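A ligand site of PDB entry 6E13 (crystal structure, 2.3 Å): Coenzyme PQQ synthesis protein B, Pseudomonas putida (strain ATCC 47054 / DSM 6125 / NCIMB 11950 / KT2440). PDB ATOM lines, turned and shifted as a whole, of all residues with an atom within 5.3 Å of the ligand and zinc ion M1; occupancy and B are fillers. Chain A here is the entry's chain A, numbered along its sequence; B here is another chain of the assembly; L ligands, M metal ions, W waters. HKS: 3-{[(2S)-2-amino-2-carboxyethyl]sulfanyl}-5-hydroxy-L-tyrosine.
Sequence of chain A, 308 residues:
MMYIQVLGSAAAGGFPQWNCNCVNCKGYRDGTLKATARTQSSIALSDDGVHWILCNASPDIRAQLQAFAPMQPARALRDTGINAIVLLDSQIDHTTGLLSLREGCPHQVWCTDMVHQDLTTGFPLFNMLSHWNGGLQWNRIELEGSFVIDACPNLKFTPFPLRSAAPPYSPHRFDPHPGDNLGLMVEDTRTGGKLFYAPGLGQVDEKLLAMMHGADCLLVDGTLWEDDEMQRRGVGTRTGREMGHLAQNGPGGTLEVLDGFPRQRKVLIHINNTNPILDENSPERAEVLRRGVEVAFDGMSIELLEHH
Within 4 Å of zinc ion M1: Cys 20, Cys 22, Cys 25 and Asn 273. The nearest printed residue that does not touch zinc ion M1 is Thr 274 (4.6 Å).
The side-chain sulfur (SD) of Met 230 sits close to an oxygen (O03) of the ligand, 3.7 Å away. Residues that only touch the ligand: Ala 11, Asp 93, Pro 168, Met 243, His 270 and Arg 102 of chain B. Hydrophobic or aromatic side chains within 4 Å of the ligand: Ala 11, Ala 12, Pro 168, Met 230, Met 243, His 270 and Trp 132 of chain B. Within 4 Å of the ligand: Ala 11, Ala 12, Gln 17, Gln 91, Asp 93, Pro 168, Met 230, Met 243, His 270, Asn 272, Asn 273, Arg 78 of chain B, Arg 102 of chain B and Trp 132 of chain B. The nearest printed residue that does not touch the ligand is His 245 (4.03 Å).
OD1 of Asn 273 is bound to zinc ion M1, at 2.1 Å. Zinc ion M1 is bound by the side-chain sulfur (SG) of Cys 20 (2.3 Å). Zinc ion M1 is bound by the side-chain sulfur (SG) of Cys 25, at 2.3 Å. Zinc ion M1 is bound by SG of Cys 22 (2.4 Å).
O of Met 230 is in hydrogen-bond range of N of Val 235 (3.2 Å). The side-chain amide oxygen (OE1) of Gln 17 lies within hydrogen-bond range of the backbone NH (N) of Gly 13. O of His 270 sits close to N of Thr 223. The backbone NH (N) of Asn 272 sits at hydrogen-bond distance from the backbone carbonyl oxygen (O) of Thr 223 (3.0 Å). The side-chain sulfur of Cys 22 sits close to the backbone NH of Asn 24 (3.4 Å). The side-chain amide oxygen of Gln 17 sits at hydrogen-bond distance from the side-chain amide nitrogen of Asn 273, at 2.8 Å. NE of Arg 78 of chain B sits close to SG of Cys 20 (3.4 Å). The guanidinium group (NH1) of Arg 78 of chain B sits close to the side-chain amide nitrogen (NE2) of Gln 17.
The backbone NH (N) of Ala 12 sits at hydrogen-bond distance from an oxygen (O20) of the ligand. ND2 of Asn 273 is in hydrogen-bond range of O03 of the ligand (3.1 Å). The guanidinium group (NH1) of Arg 78 of chain B lies within salt-bridge range of an oxygen (O01) of the ligand (2.6 Å). N16 of the ligand sits close to NE1 of Trp 132 of chain B, at 3.3 Å. OE1 of Gln 91 sits close to O15 of the ligand, 3.1 Å away. OD1 of Asn 272 is in hydrogen-bond range of N05 of the ligand (2.8 Å). OE1 of Gln 17 is in hydrogen-bond range of N05 of the ligand.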
ATOM      1  N   ALA A  11      -0.011   4.169  -1.253  1.00  0.00           N
ATOM      2  CA  ALA A  11       0.991   4.660  -2.191  1.00  0.00           C
ATOM      3  C   ALA A  11       1.597   3.447  -2.907  1.00  0.00           C
ATOM      4  O   ALA A  11       1.141   2.311  -2.746  1.00  0.00           O
ATOM      5  CB  ALA A  11       2.037   5.472  -1.423  1.00  0.00           C
ATOM      6  N   ALA A  12       2.607   3.677  -3.754  1.00  0.00           N
ATOM      7  CA  ALA A  12       3.784   2.820  -3.675  1.00  0.00           C
ATOM      8  C   ALA A  12       3.711   1.360  -4.097  1.00  0.00           C
ATOM      9  O   ALA A  12       3.408   1.028  -5.241  1.00  0.00           O
ATOM     10  CB  ALA A  12       4.231   2.742  -2.227  1.00  0.00           C
ATOM     11  N   GLY A  13       4.081   0.496  -3.178  1.00  0.00           N
ATOM     12  CA  GLY A  13       4.027  -0.941  -3.374  1.00  0.00           C
ATOM     13  C   GLY A  13       2.893  -1.491  -2.553  1.00  0.00           C
ATOM     14  O   GLY A  13       2.887  -2.668  -2.180  1.00  0.00           O
ATOM     15  N   GLN A  17       3.823  -3.965   1.515  1.00  0.00           N
ATOM     16  CA  GLN A  17       4.659  -3.944   0.321  1.00  0.00           C
ATOM     17  C   GLN A  17       5.450  -5.249   0.221  1.00  0.00           C
ATOM     18  O   GLN A  17       5.986  -5.743   1.216  1.00  0.00           O
ATOM     19  CB  GLN A  17       5.600  -2.740   0.345  1.00  0.00           C
ATOM     20  CG  GLN A  17       6.513  -2.599  -0.850  1.00  0.00           C
ATOM     21  CD  GLN A  17       7.141  -1.195  -0.892  1.00  0.00           C
ATOM     22  OE1 GLN A  17       6.416  -0.190  -0.852  1.00  0.00           O
ATOM     23  NE2 GLN A  17       8.471  -1.123  -0.960  1.00  0.00           N
ATOM     24  N   CYS A  20       8.967  -5.525   1.940  1.00  0.00           N
ATOM     25  CA  CYS A  20       9.174  -4.653   3.095  1.00  0.00           C
ATOM     26  C   CYS A  20       8.826  -5.383   4.377  1.00  0.00           C
ATOM     27  O   CYS A  20       7.768  -5.999   4.490  1.00  0.00           O
ATOM     28  CB  CYS A  20       8.311  -3.395   2.994  1.00  0.00           C
ATOM     29  SG  CYS A  20       8.627  -2.253   4.367  1.00  0.00           S
ATOM     30  N   ASN A  21       9.719  -5.271   5.361  1.00  0.00           N
ATOM     31  CA  ASN A  21       9.487  -5.813   6.697  1.00  0.00           C
ATOM     32  C   ASN A  21       9.613  -4.720   7.754  1.00  0.00           C
ATOM     33  O   ASN A  21      10.109  -4.947   8.859  1.00  0.00           O
ATOM     34  CB  ASN A  21      10.435  -6.977   6.967  1.00  0.00           C
ATOM     35  CG  ASN A  21      10.240  -8.126   5.982  1.00  0.00           C
ATOM     36  OD1 ASN A  21       9.256  -8.861   6.055  1.00  0.00           O
ATOM     37  ND2 ASN A  21      11.192  -8.278   5.053  1.00  0.00           N
ATOM     38  N   CYS A  22       9.158  -3.512   7.403  1.00  0.00           N
ATOM     39  CA  CYS A  22       9.075  -2.401   8.340  1.00  0.00           C
ATOM     40  C   CYS A  22       8.050  -2.731   9.427  1.00  0.00           C
ATOM     41  O   CYS A  22       7.353  -3.749   9.376  1.00  0.00           O
ATOM     42  CB  CYS A  22       8.708  -1.111   7.612  1.00  0.00           C
ATOM     43  SG  CYS A  22       6.886  -0.881   7.352  1.00  0.00           S
ATOM     44  N   ASN A  24       5.148  -1.582  10.184  1.00  0.00           N
ATOM     45  CA  ASN A  24       3.785  -1.759   9.695  1.00  0.00           C
ATOM     46  C   ASN A  24       3.603  -3.069   8.925  1.00  0.00           C
ATOM     47  O   ASN A  24       2.673  -3.836   9.190  1.00  0.00           O
ATOM     48  CB  ASN A  24       3.386  -0.593   8.797  1.00  0.00           C
ATOM     49  CG  ASN A  24       2.910   0.627   9.562  1.00  0.00           C
ATOM     50  OD1 ASN A  24       2.538   0.534  10.731  1.00  0.00           O
ATOM     51  ND2 ASN A  24       2.907   1.789   8.889  1.00  0.00           N
ATOM     52  N   CYS A  25       4.491  -3.333   7.954  1.00  0.00           N
ATOM     53  CA  CYS A  25       4.272  -4.474   7.051  1.00  0.00           C
ATOM     54  C   CYS A  25       4.471  -5.807   7.770  1.00  0.00           C
ATOM     55  O   CYS A  25       3.627  -6.714   7.666  1.00  0.00           O
ATOM     56  CB  CYS A  25       5.193  -4.367   5.834  1.00  0.00           C
ATOM     57  SG  CYS A  25       4.754  -3.008   4.673  1.00  0.00           S
ATOM     58  N   GLN A  91       3.424   8.110 -14.038  1.00  0.00           N
ATOM     59  CA  GLN A  91       4.221   7.192 -13.225  1.00  0.00           C
ATOM     60  C   GLN A  91       3.756   5.753 -13.420  1.00  0.00           C
ATOM     61  O   GLN A  91       2.590   5.466 -13.696  1.00  0.00           O
ATOM     62  CB  GLN A  91       4.149   7.598 -11.746  1.00  0.00           C
ATOM     63  CG  GLN A  91       4.787   8.939 -11.511  1.00  0.00           C
ATOM     64  CD  GLN A  91       4.453   9.525 -10.156  1.00  0.00           C
ATOM     65  OE1 GLN A  91       4.180   8.804  -9.207  1.00  0.00           O
ATOM     66  NE2 GLN A  91       4.467  10.854 -10.059  1.00  0.00           N
ATOM     67  N   ILE A  92       4.712   4.842 -13.299  1.00  0.00           N
ATOM     68  CA  ILE A  92       4.419   3.422 -13.418  1.00  0.00           C
ATOM     69  C   ILE A  92       3.339   3.032 -12.423  1.00  0.00           C
ATOM     70  O   ILE A  92       2.392   2.328 -12.774  1.00  0.00           O
ATOM     71  CB  ILE A  92       5.715   2.627 -13.239  1.00  0.00           C
ATOM     72  CG1 ILE A  92       6.649   2.903 -14.429  1.00  0.00           C
ATOM     73  CG2 ILE A  92       5.470   1.144 -13.024  1.00  0.00           C
ATOM     74  CD1 ILE A  92       8.027   2.472 -14.190  1.00  0.00           C
ATOM     75  N   ASP A  93       3.438   3.541 -11.194  1.00  0.00           N
ATOM     76  CA  ASP A  93       2.479   3.189 -10.148  1.00  0.00           C
ATOM     77  C   ASP A  93       1.047   3.533 -10.552  1.00  0.00           C
ATOM     78  O   ASP A  93       0.097   2.906 -10.081  1.00  0.00           O
ATOM     79  CB  ASP A  93       2.825   3.913  -8.843  1.00  0.00           C
ATOM     80  CG  ASP A  93       3.975   3.257  -8.090  1.00  0.00           C
ATOM     81  OD1 ASP A  93       4.158   2.027  -8.221  1.00  0.00           O
ATOM     82  OD2 ASP A  93       4.711   3.966  -7.362  1.00  0.00           O
ATOM     83  N   PRO A 167       8.584  11.176 -14.328  1.00  0.00           N
ATOM     84  CA  PRO A 167       9.079   9.888 -13.753  1.00  0.00           C
ATOM     85  C   PRO A 167      10.496   9.554 -14.185  1.00  0.00           C
ATOM     86  O   PRO A 167      10.961  10.032 -15.227  1.00  0.00           O
ATOM     87  CB  PRO A 167       8.083   8.860 -14.309  1.00  0.00           C
ATOM     88  CG  PRO A 167       6.915   9.649 -14.773  1.00  0.00           C
ATOM     89  CD  PRO A 167       7.425  10.982 -15.195  1.00  0.00           C
ATOM     90  N   PRO A 168      11.172   8.653 -13.448  1.00  0.00           N
ATOM     91  CA  PRO A 168      12.593   8.351 -13.754  1.00  0.00           C
ATOM     92  C   PRO A 168      12.831   7.758 -15.133  1.00  0.00           C
ATOM     93  O   PRO A 168      13.926   7.928 -15.687  1.00  0.00           O
ATOM     94  CB  PRO A 168      12.978   7.340 -12.658  1.00  0.00           C
ATOM     95  CG  PRO A 168      11.968   7.568 -11.556  1.00  0.00           C
ATOM     96  CD  PRO A 168      10.707   7.970 -12.234  1.00  0.00           C
ATOM     97  N   THR A 223       0.920  10.281   1.939  1.00  0.00           N
ATOM     98  CA  THR A 223       1.794   9.118   1.842  1.00  0.00           C
ATOM     99  C   THR A 223       2.727   9.017   3.053  1.00  0.00           C
ATOM    100  O   THR A 223       2.934   7.922   3.575  1.00  0.00           O
ATOM    101  CB  THR A 223       2.573   9.102   0.522  1.00  0.00           C
ATOM    102  OG1 THR A 223       3.972   9.298   0.743  1.00  0.00           O
ATOM    103  CG2 THR A 223       2.075  10.122  -0.441  1.00  0.00           C
ATOM    104  N   MET A 230      11.130   7.452   5.620  1.00  0.00           N
ATOM    105  CA  MET A 230      11.887   6.311   5.128  1.00  0.00           C
ATOM    106  C   MET A 230      13.111   6.035   6.011  1.00  0.00           C
ATOM    107  O   MET A 230      13.380   4.894   6.401  1.00  0.00           O
ATOM    108  CB  MET A 230      12.315   6.522   3.673  1.00  0.00           C
ATOM    109  CG  MET A 230      11.172   6.636   2.693  1.00  0.00           C
ATOM    110  SD  MET A 230      10.335   5.067   2.388  1.00  0.00           S
ATOM    111  CE  MET A 230      11.386   4.321   1.143  1.00  0.00           C
ATOM    112  N   VAL A 235      14.147   1.877   5.887  1.00  0.00           N
ATOM    113  CA  VAL A 235      13.822   1.261   4.599  1.00  0.00           C
ATOM    114  C   VAL A 235      14.367   2.035   3.406  1.00  0.00           C
ATOM    115  O   VAL A 235      14.311   1.526   2.274  1.00  0.00           O
ATOM    116  CB  VAL A 235      12.312   1.043   4.449  1.00  0.00           C
ATOM    117  CG1 VAL A 235      11.850  -0.049   5.401  1.00  0.00           C
ATOM    118  CG2 VAL A 235      11.571   2.348   4.709  1.00  0.00           C
ATOM    119  N   MET A 243      10.316  12.971  -3.215  1.00  0.00           N
ATOM    120  CA  MET A 243       9.280  12.270  -3.952  1.00  0.00           C
ATOM    121  C   MET A 243       8.126  13.166  -4.366  1.00  0.00           C
ATOM    122  O   MET A 243       7.206  12.686  -5.050  1.00  0.00           O
ATOM    123  CB  MET A 243       8.706  11.117  -3.133  1.00  0.00           C
ATOM    124  CG  MET A 243       9.720  10.165  -2.546  1.00  0.00           C
ATOM    125  SD  MET A 243       8.936   9.182  -1.258  1.00  0.00           S
ATOM    126  CE  MET A 243      10.284   8.175  -0.663  1.00  0.00           C
ATOM    127  N   HIS A 245       5.992  14.626  -2.145  1.00  0.00           N
ATOM    128  CA  HIS A 245       4.941  14.296  -1.201  1.00  0.00           C
ATOM    129  C   HIS A 245       5.158  15.110   0.063  1.00  0.00           C
ATOM    130  O   HIS A 245       6.166  14.944   0.748  1.00  0.00           O
ATOM    131  CB  HIS A 245       4.916  12.786  -0.892  1.00  0.00           C
ATOM    132  CG  HIS A 245       4.480  11.938  -2.045  1.00  0.00           C
ATOM    133  ND1 HIS A 245       3.277  12.129  -2.703  1.00  0.00           N
ATOM    134  CD2 HIS A 245       5.069  10.882  -2.657  1.00  0.00           C
ATOM    135  CE1 HIS A 245       3.153  11.231  -3.660  1.00  0.00           C
ATOM    136  NE2 HIS A 245       4.230  10.462  -3.660  1.00  0.00           N
ATOM    137  N   HIS A 270      -3.642   7.660  -0.577  1.00  0.00           N
ATOM    138  CA  HIS A 270      -2.312   7.416  -1.145  1.00  0.00           C
ATOM    139  C   HIS A 270      -1.310   7.377   0.006  1.00  0.00           C
ATOM    140  O   HIS A 270      -0.406   8.214   0.077  1.00  0.00           O
ATOM    141  CB  HIS A 270      -1.948   8.489  -2.178  1.00  0.00           C
ATOM    142  CG  HIS A 270      -0.747   8.185  -3.013  1.00  0.00           C
ATOM    143  ND1 HIS A 270       0.537   8.501  -2.636  1.00  0.00           N
ATOM    144  CD2 HIS A 270      -0.645   7.637  -4.254  1.00  0.00           C
ATOM    145  CE1 HIS A 270       1.385   8.141  -3.584  1.00  0.00           C
ATOM    146  NE2 HIS A 270       0.696   7.616  -4.576  1.00  0.00           N
ATOM    147  N   ASN A 272       1.591   5.554   2.297  1.00  0.00           N
ATOM    148  CA  ASN A 272       2.695   4.613   2.154  1.00  0.00           C
ATOM    149  C   ASN A 272       2.720   3.582   3.277  1.00  0.00           C
ATOM    150  O   ASN A 272       2.275   3.835   4.406  1.00  0.00           O
ATOM    151  CB  ASN A 272       4.034   5.364   2.096  1.00  0.00           C
ATOM    152  CG  ASN A 272       5.165   4.493   1.563  1.00  0.00           C
ATOM    153  OD1 ASN A 272       5.227   4.191   0.373  1.00  0.00           O
ATOM    154  ND2 ASN A 272       6.078   4.132   2.444  1.00  0.00           N
ATOM    155  N   ASN A 273       3.255   2.399   2.947  1.00  0.00           N
ATOM    156  CA  ASN A 273       3.335   1.294   3.888  1.00  0.00           C
ATOM    157  C   ASN A 273       4.063   1.668   5.178  1.00  0.00           C
ATOM    158  O   ASN A 273       3.863   1.008   6.194  1.00  0.00           O
ATOM    159  CB  ASN A 273       4.011   0.080   3.232  1.00  0.00           C
ATOM    160  CG  ASN A 273       5.487   0.319   2.959  1.00  0.00           C
ATOM    161  OD1 ASN A 273       6.321   0.215   3.859  1.00  0.00           O
ATOM    162  ND2 ASN A 273       5.817   0.648   1.710  1.00  0.00           N
ATOM    163  N   THR A 274       4.903   2.708   5.152  1.00  0.00           N
ATOM    164  CA  THR A 274       5.657   3.102   6.347  1.00  0.00           C
ATOM    165  C   THR A 274       4.860   4.002   7.297  1.00  0.00           C
ATOM    166  O   THR A 274       5.305   4.213   8.427  1.00  0.00           O
ATOM    167  CB  THR A 274       6.936   3.821   5.962  1.00  0.00           C
ATOM    168  OG1 THR A 274       6.616   4.900   5.064  1.00  0.00           O
ATOM    169  CG2 THR A 274       7.935   2.858   5.312  1.00  0.00           C
ATOM    170  N   ARG B  78      14.348  -4.758   4.195  1.00  0.00           N
ATOM    171  CA  ARG B  78      13.934  -5.019   2.830  1.00  0.00           C
ATOM    172  C   ARG B  78      14.502  -6.370   2.411  1.00  0.00           C
ATOM    173  O   ARG B  78      15.709  -6.602   2.544  1.00  0.00           O
ATOM    174  CB  ARG B  78      14.376  -3.893   1.892  1.00  0.00           C
ATOM    175  CG  ARG B  78      13.613  -2.567   2.110  1.00  0.00           C
ATOM    176  CD  ARG B  78      12.157  -2.677   1.639  1.00  0.00           C
ATOM    177  NE  ARG B  78      11.199  -1.751   2.269  1.00  0.00           N
ATOM    178  CZ  ARG B  78      10.781  -0.595   1.724  1.00  0.00           C
ATOM    179  NH1 ARG B  78      11.252  -0.186   0.544  1.00  0.00           N
ATOM    180  NH2 ARG B  78       9.899   0.157   2.350  1.00  0.00           N
ATOM    181  N   ARG B 102      10.316  -3.021  -8.737  1.00  0.00           N
ATOM    182  CA  ARG B 102      11.412  -2.078  -8.910  1.00  0.00           C
ATOM    183  C   ARG B 102      11.950  -1.558  -7.590  1.00  0.00           C
ATOM    184  O   ARG B 102      13.087  -1.098  -7.543  1.00  0.00           O
ATOM    185  CB  ARG B 102      11.019  -0.900  -9.805  1.00  0.00           C
ATOM    186  CG  ARG B 102       9.749  -0.223  -9.450  1.00  0.00           C
ATOM    187  CD  ARG B 102       9.089   0.326 -10.723  1.00  0.00           C
ATOM    188  NE  ARG B 102       7.948   1.183 -10.405  1.00  0.00           N
ATOM    189  CZ  ARG B 102       6.863   0.783  -9.752  1.00  0.00           C
ATOM    190  NH1 ARG B 102       5.898   1.653  -9.521  1.00  0.00           N
ATOM    191  NH2 ARG B 102       6.729  -0.465  -9.310  1.00  0.00           N
ATOM    192  N   GLU B 103      11.178  -1.653  -6.507  1.00  0.00           N
ATOM    193  CA  GLU B 103      11.722  -1.317  -5.189  1.00  0.00           C
ATOM    194  C   GLU B 103      12.775  -2.311  -4.731  1.00  0.00           C
ATOM    195  O   GLU B 103      13.273  -2.170  -3.611  1.00  0.00           O
ATOM    196  CB  GLU B 103      10.617  -1.268  -4.121  1.00  0.00           C
ATOM    197  CG  GLU B 103       9.378  -0.427  -4.416  1.00  0.00           C
ATOM    198  CD  GLU B 103       8.323  -1.189  -5.209  1.00  0.00           C
ATOM    199  OE1 GLU B 103       7.154  -0.714  -5.256  1.00  0.00           O
ATOM    200  OE2 GLU B 103       8.686  -2.230  -5.822  1.00  0.00           O
ATOM    201  N   TRP B 132      16.073   2.140 -11.880  1.00  0.00           N
ATOM    202  CA  TRP B 132      15.852   1.826 -10.468  1.00  0.00           C
ATOM    203  C   TRP B 132      17.013   0.949 -10.039  1.00  0.00           C
ATOM    204  O   TRP B 132      16.955  -0.267 -10.211  1.00  0.00           O
ATOM    205  CB  TRP B 132      14.508   1.129 -10.222  1.00  0.00           C
ATOM    206  CG  TRP B 132      13.310   2.044 -10.142  1.00  0.00           C
ATOM    207  CD1 TRP B 132      12.677   2.462  -9.009  1.00  0.00           C
ATOM    208  CD2 TRP B 132      12.606   2.629 -11.244  1.00  0.00           C
ATOM    209  NE1 TRP B 132      11.630   3.281  -9.340  1.00  0.00           N
ATOM    210  CE2 TRP B 132      11.560   3.400 -10.707  1.00  0.00           C
ATOM    211  CE3 TRP B 132      12.763   2.588 -12.632  1.00  0.00           C
ATOM    212  CZ2 TRP B 132      10.666   4.125 -11.515  1.00  0.00           C
ATOM    213  CZ3 TRP B 132      11.865   3.297 -13.433  1.00  0.00           C
ATOM    214  CH2 TRP B 132      10.836   4.054 -12.871  1.00  0.00           C
HETATM  215  C02 HKS L   1       8.823   2.385  -0.195  1.00  0.00           C
HETATM  216  C04 HKS L   1       8.217   3.201  -1.281  1.00  0.00           C
HETATM  217  C06 HKS L   1       8.236   4.786  -1.161  1.00  0.00           C
HETATM  218  C07 HKS L   1       7.532   5.394  -2.385  1.00  0.00           C
HETATM  219  C08 HKS L   1       8.303   5.717  -3.495  1.00  0.00           C
HETATM  220  C09 HKS L   1       7.684   6.257  -4.619  1.00  0.00           C
HETATM  221  C11 HKS L   1       8.641   5.255  -7.093  1.00  0.00           C
HETATM  222  C12 HKS L   1       8.744   5.771  -8.516  1.00  0.00           C
HETATM  223  C13 HKS L   1       7.671   6.860  -8.888  1.00  0.00           C
HETATM  224  C17 HKS L   1       6.287   6.485  -4.671  1.00  0.00           C
HETATM  225  C19 HKS L   1       5.522   6.170  -3.581  1.00  0.00           C
HETATM  226  C21 HKS L   1       6.137   5.618  -2.428  1.00  0.00           C
HETATM  227  N05 HKS L   1       6.902   2.791  -1.360  1.00  0.00           N
HETATM  228  N16 HKS L   1       8.663   4.630  -9.405  1.00  0.00           N
HETATM  229  O01 HKS L   1       9.867   1.735  -0.430  1.00  0.00           O
HETATM  230  O03 HKS L   1       8.269   2.315   0.924  1.00  0.00           O
HETATM  231  O14 HKS L   1       7.978   7.731  -9.768  1.00  0.00           O
HETATM  232  O15 HKS L   1       6.514   6.884  -8.338  1.00  0.00           O
HETATM  233  O18 HKS L   1       5.560   7.037  -5.789  1.00  0.00           O
HETATM  234  O20 HKS L   1       4.135   6.438  -3.708  1.00  0.00           O
HETATM  235  S10 HKS L   1       8.733   6.629  -6.019  1.00  0.00           S
HETATM  236 ZN    ZN M   1       6.543  -1.552   5.040  1.00  0.00          ZN
HETATM  237 ZN    ZN M   2       1.371   6.384  -6.196  1.00  0.00          ZN
HETATM  238  O   HOH W   1       5.834   4.609 -10.198  1.00  0.00           O
